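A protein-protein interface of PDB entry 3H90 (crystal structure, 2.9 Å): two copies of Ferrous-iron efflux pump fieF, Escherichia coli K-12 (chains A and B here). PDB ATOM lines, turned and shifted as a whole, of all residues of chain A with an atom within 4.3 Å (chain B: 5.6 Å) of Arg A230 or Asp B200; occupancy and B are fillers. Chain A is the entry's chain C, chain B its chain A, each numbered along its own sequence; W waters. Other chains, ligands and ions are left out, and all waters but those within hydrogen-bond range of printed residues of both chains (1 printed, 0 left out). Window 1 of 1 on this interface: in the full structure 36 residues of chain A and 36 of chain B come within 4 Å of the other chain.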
ATOM      1  N   HIS A  64      -1.464  -3.274  35.062  1.00  0.00           N
ATOM      2  CA  HIS A  64      -1.904  -2.154  34.231  1.00  0.00           C
ATOM      3  C   HIS A  64      -2.801  -1.276  35.102  1.00  0.00           C
ATOM      4  O   HIS A  64      -4.020  -1.365  35.052  1.00  0.00           O
ATOM      5  CB  HIS A  64      -2.625  -2.645  32.971  1.00  0.00           C
ATOM      6  CG  HIS A  64      -1.822  -3.610  32.158  1.00  0.00           C
ATOM      7  ND1 HIS A  64      -2.037  -4.969  32.191  1.00  0.00           N
ATOM      8  CD2 HIS A  64      -0.793  -3.413  31.304  1.00  0.00           C
ATOM      9  CE1 HIS A  64      -1.177  -5.569  31.389  1.00  0.00           C
ATOM     10  NE2 HIS A  64      -0.410  -4.647  30.841  1.00  0.00           N
ATOM     11  N   PHE A  66      -3.185   1.921  35.138  1.00  0.00           N
ATOM     12  CA  PHE A  66      -3.940   2.815  34.272  1.00  0.00           C
ATOM     13  C   PHE A  66      -4.750   1.917  33.334  1.00  0.00           C
ATOM     14  O   PHE A  66      -4.991   0.761  33.656  1.00  0.00           O
ATOM     15  CB  PHE A  66      -2.985   3.756  33.536  1.00  0.00           C
ATOM     16  CG  PHE A  66      -2.210   4.651  34.459  1.00  0.00           C
ATOM     17  CD1 PHE A  66      -2.642   5.944  34.717  1.00  0.00           C
ATOM     18  CD2 PHE A  66      -1.067   4.195  35.099  1.00  0.00           C
ATOM     19  CE1 PHE A  66      -1.937   6.777  35.589  1.00  0.00           C
ATOM     20  CE2 PHE A  66      -0.361   5.018  35.967  1.00  0.00           C
ATOM     21  CZ  PHE A  66      -0.795   6.308  36.213  1.00  0.00           C
ATOM     22  N   LYS A  70      -4.633   1.943  25.454  1.00  0.00           N
ATOM     23  CA  LYS A  70      -3.588   1.944  24.425  1.00  0.00           C
ATOM     24  C   LYS A  70      -3.608   0.754  23.454  1.00  0.00           C
ATOM     25  O   LYS A  70      -3.170   0.875  22.308  1.00  0.00           O
ATOM     26  CB  LYS A  70      -2.217   2.039  25.080  1.00  0.00           C
ATOM     27  CG  LYS A  70      -2.053   3.217  26.000  1.00  0.00           C
ATOM     28  CD  LYS A  70      -1.666   4.464  25.235  1.00  0.00           C
ATOM     29  CE  LYS A  70      -1.247   5.560  26.213  1.00  0.00           C
ATOM     30  NZ  LYS A  70      -0.050   5.148  27.013  1.00  0.00           N
ATOM     31  N   ASP A 200       2.523  10.137  24.867  1.00  0.00           N
ATOM     32  CA  ASP A 200       1.362  10.596  25.611  1.00  0.00           C
ATOM     33  C   ASP A 200       1.035  12.029  25.246  1.00  0.00           C
ATOM     34  O   ASP A 200       1.340  12.958  26.010  1.00  0.00           O
ATOM     35  CB  ASP A 200       1.520  10.398  27.125  1.00  0.00           C
ATOM     36  CG  ASP A 200       1.281   8.947  27.555  1.00  0.00           C
ATOM     37  OD1 ASP A 200       2.017   8.459  28.445  1.00  0.00           O
ATOM     38  OD2 ASP A 200       0.366   8.296  27.000  1.00  0.00           O
ATOM     39  N   ARG A 201       0.413  12.201  24.077  1.00  0.00           N
ATOM     40  CA  ARG A 201       0.058  13.526  23.568  1.00  0.00           C
ATOM     41  C   ARG A 201      -1.122  14.098  24.315  1.00  0.00           C
ATOM     42  O   ARG A 201      -2.040  13.367  24.675  1.00  0.00           O
ATOM     43  CB  ARG A 201      -0.246  13.505  22.067  1.00  0.00           C
ATOM     44  CG  ARG A 201      -0.844  14.818  21.559  1.00  0.00           C
ATOM     45  CD  ARG A 201      -1.382  14.758  20.140  1.00  0.00           C
ATOM     46  NE  ARG A 201      -0.422  15.290  19.173  1.00  0.00           N
ATOM     47  CZ  ARG A 201      -0.219  16.585  18.923  1.00  0.00           C
ATOM     48  NH1 ARG A 201      -0.905  17.525  19.576  1.00  0.00           N
ATOM     49  NH2 ARG A 201       0.685  16.944  18.016  1.00  0.00           N
ATOM     50  N   LEU A 203      -4.520  16.494  25.278  1.00  0.00           N
ATOM     51  CA  LEU A 203      -5.880  16.595  24.754  1.00  0.00           C
ATOM     52  C   LEU A 203      -6.014  17.760  23.743  1.00  0.00           C
ATOM     53  O   LEU A 203      -5.179  18.674  23.724  1.00  0.00           O
ATOM     54  CB  LEU A 203      -6.878  16.750  25.916  1.00  0.00           C
ATOM     55  CG  LEU A 203      -7.127  15.593  26.891  1.00  0.00           C
ATOM     56  CD1 LEU A 203      -8.084  16.014  27.969  1.00  0.00           C
ATOM     57  CD2 LEU A 203      -7.676  14.381  26.186  1.00  0.00           C
ATOM     58  N   THR A 229      -2.441  16.358  30.545  1.00  0.00           N
ATOM     59  CA  THR A 229      -3.562  15.705  29.912  1.00  0.00           C
ATOM     60  C   THR A 229      -3.096  14.675  28.888  1.00  0.00           C
ATOM     61  O   THR A 229      -2.024  14.802  28.296  1.00  0.00           O
ATOM     62  CB  THR A 229      -4.438  16.743  29.194  1.00  0.00           C
ATOM     63  OG1 THR A 229      -3.590  17.628  28.446  1.00  0.00           O
ATOM     64  CG2 THR A 229      -5.288  17.549  30.204  1.00  0.00           C
ATOM     65  N   ARG A 230      -3.924  13.659  28.688  1.00  0.00           N
ATOM     66  CA  ARG A 230      -3.685  12.603  27.725  1.00  0.00           C
ATOM     67  C   ARG A 230      -4.900  11.696  27.765  1.00  0.00           C
ATOM     68  O   ARG A 230      -5.626  11.682  28.757  1.00  0.00           O
ATOM     69  CB  ARG A 230      -2.438  11.800  28.102  1.00  0.00           C
ATOM     70  CG  ARG A 230      -2.495  11.135  29.485  1.00  0.00           C
ATOM     71  CD  ARG A 230      -1.181  10.480  29.849  1.00  0.00           C
ATOM     72  NE  ARG A 230      -1.251   9.024  29.945  1.00  0.00           N
ATOM     73  CZ  ARG A 230      -1.453   8.356  31.083  1.00  0.00           C
ATOM     74  NH1 ARG A 230      -1.637   9.014  32.227  1.00  0.00           N
ATOM     75  NH2 ARG A 230      -1.481   7.025  31.081  1.00  0.00           N
ATOM     76  N   GLN A 231      -5.141  10.936  26.706  1.00  0.00           N
ATOM     77  CA  GLN A 231      -6.087   9.847  26.850  1.00  0.00           C
ATOM     78  C   GLN A 231      -5.539   8.571  26.297  1.00  0.00           C
ATOM     79  O   GLN A 231      -4.780   8.585  25.337  1.00  0.00           O
ATOM     80  CB  GLN A 231      -7.452  10.162  26.253  1.00  0.00           C
ATOM     81  CG  GLN A 231      -7.493  10.450  24.767  1.00  0.00           C
ATOM     82  CD  GLN A 231      -8.860  10.949  24.345  1.00  0.00           C
ATOM     83  OE1 GLN A 231      -9.028  12.118  23.987  1.00  0.00           O
ATOM     84  NE2 GLN A 231      -9.854  10.073  24.415  1.00  0.00           N
ATOM     85  N   ARG A 236      -9.786   9.533  29.538  1.00  0.00           N
ATOM     86  CA  ARG A 236      -8.798  10.602  29.527  1.00  0.00           C
ATOM     87  C   ARG A 236      -8.201  10.841  30.899  1.00  0.00           C
ATOM     88  O   ARG A 236      -8.905  10.796  31.912  1.00  0.00           O
ATOM     89  CB  ARG A 236      -9.433  11.905  29.067  1.00  0.00           C
ATOM     90  CG  ARG A 236     -10.604  11.734  28.171  1.00  0.00           C
ATOM     91  CD  ARG A 236     -11.307  13.055  27.986  1.00  0.00           C
ATOM     92  NE  ARG A 236     -12.649  12.828  27.463  1.00  0.00           N
ATOM     93  CZ  ARG A 236     -12.950  12.779  26.172  1.00  0.00           C
ATOM     94  NH1 ARG A 236     -12.014  12.970  25.253  1.00  0.00           N
ATOM     95  NH2 ARG A 236     -14.197  12.545  25.803  1.00  0.00           N
ATOM     96  N   PHE A 237      -6.909  11.138  30.930  1.00  0.00           N
ATOM     97  CA  PHE A 237      -6.204  11.341  32.191  1.00  0.00           C
ATOM     98  C   PHE A 237      -5.861  12.805  32.409  1.00  0.00           C
ATOM     99  O   PHE A 237      -5.274  13.463  31.545  1.00  0.00           O
ATOM    100  CB  PHE A 237      -4.965  10.442  32.270  1.00  0.00           C
ATOM    101  CG  PHE A 237      -5.295   8.987  32.262  1.00  0.00           C
ATOM    102  CD1 PHE A 237      -5.330   8.278  31.071  1.00  0.00           C
ATOM    103  CD2 PHE A 237      -5.622   8.332  33.442  1.00  0.00           C
ATOM    104  CE1 PHE A 237      -5.665   6.932  31.052  1.00  0.00           C
ATOM    105  CE2 PHE A 237      -5.953   6.977  33.442  1.00  0.00           C
ATOM    106  CZ  PHE A 237      -5.971   6.274  32.242  1.00  0.00           C
ATOM    107  N   PHE B  66       3.602  15.096  29.322  1.00  0.00           N
ATOM    108  CA  PHE B  66       4.425  14.050  29.916  1.00  0.00           C
ATOM    109  C   PHE B  66       5.684  13.918  29.042  1.00  0.00           C
ATOM    110  O   PHE B  66       6.045  14.846  28.331  1.00  0.00           O
ATOM    111  CB  PHE B  66       3.615  12.753  30.020  1.00  0.00           C
ATOM    112  CG  PHE B  66       2.404  12.878  30.909  1.00  0.00           C
ATOM    113  CD1 PHE B  66       2.452  12.473  32.228  1.00  0.00           C
ATOM    114  CD2 PHE B  66       1.226  13.426  30.432  1.00  0.00           C
ATOM    115  CE1 PHE B  66       1.336  12.601  33.051  1.00  0.00           C
ATOM    116  CE2 PHE B  66       0.117  13.556  31.240  1.00  0.00           C
ATOM    117  CZ  PHE B  66       0.168  13.145  32.551  1.00  0.00           C
ATOM    118  N   LYS B  70       8.238   7.415  25.410  1.00  0.00           N
ATOM    119  CA  LYS B  70       7.634   6.336  24.621  1.00  0.00           C
ATOM    120  C   LYS B  70       8.211   6.169  23.208  1.00  0.00           C
ATOM    121  O   LYS B  70       8.152   5.075  22.623  1.00  0.00           O
ATOM    122  CB  LYS B  70       6.130   6.544  24.527  1.00  0.00           C
ATOM    123  CG  LYS B  70       5.443   6.628  25.851  1.00  0.00           C
ATOM    124  CD  LYS B  70       5.129   5.243  26.413  1.00  0.00           C
ATOM    125  CE  LYS B  70       4.162   5.337  27.608  1.00  0.00           C
ATOM    126  NZ  LYS B  70       2.866   5.994  27.220  1.00  0.00           N
ATOM    127  N   GLN B 196       4.447  -3.592  25.946  1.00  0.00           N
ATOM    128  CA  GLN B 196       4.081  -3.645  27.335  1.00  0.00           C
ATOM    129  C   GLN B 196       4.358  -2.319  28.053  1.00  0.00           C
ATOM    130  O   GLN B 196       3.767  -2.055  29.080  1.00  0.00           O
ATOM    131  CB  GLN B 196       4.785  -4.830  27.982  1.00  0.00           C
ATOM    132  CG  GLN B 196       4.055  -5.433  29.151  1.00  0.00           C
ATOM    133  CD  GLN B 196       2.638  -5.866  28.853  1.00  0.00           C
ATOM    134  OE1 GLN B 196       1.725  -5.565  29.625  1.00  0.00           O
ATOM    135  NE2 GLN B 196       2.444  -6.588  27.751  1.00  0.00           N
ATOM    136  N   SER B 197       5.240  -1.490  27.494  1.00  0.00           N
ATOM    137  CA  SER B 197       5.560  -0.175  28.062  1.00  0.00           C
ATOM    138  C   SER B 197       4.699   0.817  27.353  1.00  0.00           C
ATOM    139  O   SER B 197       4.486   1.935  27.856  1.00  0.00           O
ATOM    140  CB  SER B 197       7.017   0.232  27.823  1.00  0.00           C
ATOM    141  OG  SER B 197       7.786  -0.819  27.249  1.00  0.00           O
ATOM    142  N   LEU B 198       4.225   0.406  26.172  1.00  0.00           N
ATOM    143  CA  LEU B 198       3.293   1.198  25.384  1.00  0.00           C
ATOM    144  C   LEU B 198       1.893   1.135  25.965  1.00  0.00           C
ATOM    145  O   LEU B 198       1.236   2.177  26.064  1.00  0.00           O
ATOM    146  CB  LEU B 198       3.319   0.804  23.916  1.00  0.00           C
ATOM    147  CG  LEU B 198       4.602   1.254  23.211  1.00  0.00           C
ATOM    148  CD1 LEU B 198       4.631   0.750  21.763  1.00  0.00           C
ATOM    149  CD2 LEU B 198       4.814   2.777  23.298  1.00  0.00           C
ATOM    150  N   LEU B 199       1.439  -0.061  26.360  1.00  0.00           N
ATOM    151  CA  LEU B 199       0.377  -0.164  27.370  1.00  0.00           C
ATOM    152  C   LEU B 199       0.984   0.476  28.611  1.00  0.00           C
ATOM    153  O   LEU B 199       2.178   0.347  28.837  1.00  0.00           O
ATOM    154  CB  LEU B 199       0.070  -1.621  27.683  1.00  0.00           C
ATOM    155  CG  LEU B 199      -0.753  -2.543  26.797  1.00  0.00           C
ATOM    156  CD1 LEU B 199      -0.939  -1.990  25.402  1.00  0.00           C
ATOM    157  CD2 LEU B 199      -0.082  -3.910  26.750  1.00  0.00           C
ATOM    158  N   ASP B 200       0.241   1.176  29.434  1.00  0.00           N
ATOM    159  CA  ASP B 200       0.957   1.758  30.547  1.00  0.00           C
ATOM    160  C   ASP B 200       1.107   0.744  31.664  1.00  0.00           C
ATOM    161  O   ASP B 200       0.364   0.791  32.649  1.00  0.00           O
ATOM    162  CB  ASP B 200       0.314   3.060  31.026  1.00  0.00           C
ATOM    163  CG  ASP B 200       0.686   4.253  30.146  1.00  0.00           C
ATOM    164  OD1 ASP B 200      -0.189   5.128  29.909  1.00  0.00           O
ATOM    165  OD2 ASP B 200       1.855   4.302  29.692  1.00  0.00           O
ATOM    166  N   ARG B 201       2.071  -0.168  31.511  1.00  0.00           N
ATOM    167  CA  ARG B 201       2.286  -1.229  32.496  1.00  0.00           C
ATOM    168  C   ARG B 201       2.995  -0.711  33.726  1.00  0.00           C
ATOM    169  O   ARG B 201       3.879   0.135  33.621  1.00  0.00           O
ATOM    170  CB  ARG B 201       3.072  -2.406  31.913  1.00  0.00           C
ATOM    171  CG  ARG B 201       3.525  -3.411  32.967  1.00  0.00           C
ATOM    172  CD  ARG B 201       4.487  -4.449  32.441  1.00  0.00           C
ATOM    173  NE  ARG B 201       3.818  -5.714  32.127  1.00  0.00           N
ATOM    174  CZ  ARG B 201       3.475  -6.648  33.018  1.00  0.00           C
ATOM    175  NH1 ARG B 201       3.714  -6.480  34.319  1.00  0.00           N
ATOM    176  NH2 ARG B 201       2.880  -7.761  32.606  1.00  0.00           N
ATOM    177  N   ALA B 202       2.614  -1.253  34.880  1.00  0.00           N
ATOM    178  CA  ALA B 202       3.181  -0.896  36.181  1.00  0.00           C
ATOM    179  C   ALA B 202       4.674  -1.186  36.318  1.00  0.00           C
ATOM    180  O   ALA B 202       5.247  -1.952  35.543  1.00  0.00           O
ATOM    181  CB  ALA B 202       2.415  -1.597  37.284  1.00  0.00           C
ATOM    182  N   THR B 229       1.611   3.460  38.872  1.00  0.00           N
ATOM    183  CA  THR B 229       2.983   3.511  38.403  1.00  0.00           C
ATOM    184  C   THR B 229       3.111   3.113  36.925  1.00  0.00           C
ATOM    185  O   THR B 229       2.302   2.351  36.379  1.00  0.00           O
ATOM    186  CB  THR B 229       3.846   2.544  39.223  1.00  0.00           C
ATOM    187  OG1 THR B 229       3.173   1.273  39.321  1.00  0.00           O
ATOM    188  CG2 THR B 229       4.102   3.109  40.619  1.00  0.00           C
ATOM    189  N   ARG B 230       4.148   3.640  36.293  1.00  0.00           N
ATOM    190  CA  ARG B 230       4.471   3.365  34.906  1.00  0.00           C
ATOM    191  C   ARG B 230       5.756   4.109  34.632  1.00  0.00           C
ATOM    192  O   ARG B 230       6.096   5.048  35.365  1.00  0.00           O
ATOM    193  CB  ARG B 230       3.371   3.882  33.965  1.00  0.00           C
ATOM    194  CG  ARG B 230       3.058   5.377  34.102  1.00  0.00           C
ATOM    195  CD  ARG B 230       1.876   5.784  33.255  1.00  0.00           C
ATOM    196  NE  ARG B 230       2.216   6.654  32.123  1.00  0.00           N
ATOM    197  CZ  ARG B 230       2.190   7.987  32.162  1.00  0.00           C
ATOM    198  NH1 ARG B 230       1.868   8.639  33.280  1.00  0.00           N
ATOM    199  NH2 ARG B 230       2.492   8.677  31.075  1.00  0.00           N
ATOM    200  N   GLN B 231       6.481   3.702  33.596  1.00  0.00           N
ATOM    201  CA  GLN B 231       7.526   4.573  33.086  1.00  0.00           C
ATOM    202  C   GLN B 231       7.430   4.731  31.601  1.00  0.00           C
ATOM    203  O   GLN B 231       7.022   3.815  30.922  1.00  0.00           O
ATOM    204  CB  GLN B 231       8.928   4.159  33.525  1.00  0.00           C
ATOM    205  CG  GLN B 231       9.410   2.800  33.086  1.00  0.00           C
ATOM    206  CD  GLN B 231      10.715   2.423  33.783  1.00  0.00           C
ATOM    207  OE1 GLN B 231      10.752   1.515  34.628  1.00  0.00           O
ATOM    208  NE2 GLN B 231      11.787   3.138  33.453  1.00  0.00           N
HETATM  209  O   HOH W   1      -0.304  10.233  35.098  1.00  0.00           O
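Phe A66 touches Thr B229, and with the chains exchanged Thr A229 touches Phe B66.
Phe A66 touches Arg B230, and with the chains exchanged Arg A230 touches Phe B66.
Lys A70 touches Asp B200, and with the chains exchanged Asp A200 touches Lys B70.
Asp A200 touches Arg B230, and with the chains exchanged Arg A230 touches Asp B200.
Among the printed residues, merely in contact across the chains: His A64 with Arg B201 (3.96 Å), Phe A66 with Thr B229 (3.8 Å), Phe A66 with Arg B230 (3.6 Å), Thr A229 with Phe B66 (3.8 Å), Arg A230 with Phe B66 (3.6 Å) and Arg A230 with Arg B230 (3.7 Å).
Water W1 lies within hydrogen-bond range of the guanidinium group (NH1) of Arg B230 and the guanidinium group (NH1) of Arg A230.
The side-chain amino group of Lys B70 lies within salt-bridge range of the side-chain carboxylate of Asp A200 (2.9 Å).
The side-chain amide oxygen (OE1) of Gln B196 sits at hydrogen-bond distance from a ring nitrogen (NE2) of His A64, 2.6 Å away.
NZ of Lys A70 is in hydrogen-bond range of O of Leu B198, at 3.4 Å.
OD1 of Asp B200 lies within salt-bridge range of NZ of Lys A70, at 2.9 Å.
OD1 of Asp B200 lies within salt-bridge range of NH2 of Arg A230 (2.6 Å).
The side-chain carboxylate (OD1) of Asp A200 lies within salt-bridge range of the guanidinium group (NH2) of Arg B230.
NZ of Lys B70 lies close to NZ of Lys A70 (3.0 Å).
Of chain A, only Lys A70 and Arg A230 come within 4 Å of Asp B200.
Printed residues of chain B within 4 Å of His A64: Gln B196 and Arg B201.
Of the printed residues of chain B, Thr A229 touches Phe B66 (3.8 Å).
Printed residues of chain A within 4 Å of Leu B198: Lys A70 (3.4 Å).
Printed residues of chain A within 4 Å of Gln B196: His A64 (2.6 Å).
Arg A236 touches none of the printed residues of chain B.
Ser B197 touches none of the printed residues of chain A.
The nearest printed residue of chain B that does not touch Arg A230 is Lys B70 (5.8 Å).
The nearest residue of chain A that does not touch Asp B200 is His A64 (4.04 Å).
Of the 12 printed residues of chain B, 8 touch a printed residue of chain A.
Of the 11 printed residues of chain A, 6 touch a printed residue of chain B.
Printed residues of chain A that touch a printed residue of chain B: His A64, Phe A66, Lys A70, Asp A200, Thr A229 and Arg A230.
The side-chain amino group of Lys B70 is in salt-bridge range of the side-chain carboxylate of Asp B200.
OD2 of Asp B200 is in salt-bridge range of NE of Arg B230 (3.4 Å).
NZ of Lys A70 is in salt-bridge range of OD2 of Asp A200 (3.2 Å).
NE of Arg A230 lies within salt-bridge range of OD2 of Asp A200.
OG1 of Thr A229 is in hydrogen-bond range of N of Leu A203 (3.5 Å).
N of Phe A237 sits at hydrogen-bond distance from O of Arg A230 (2.6 Å).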
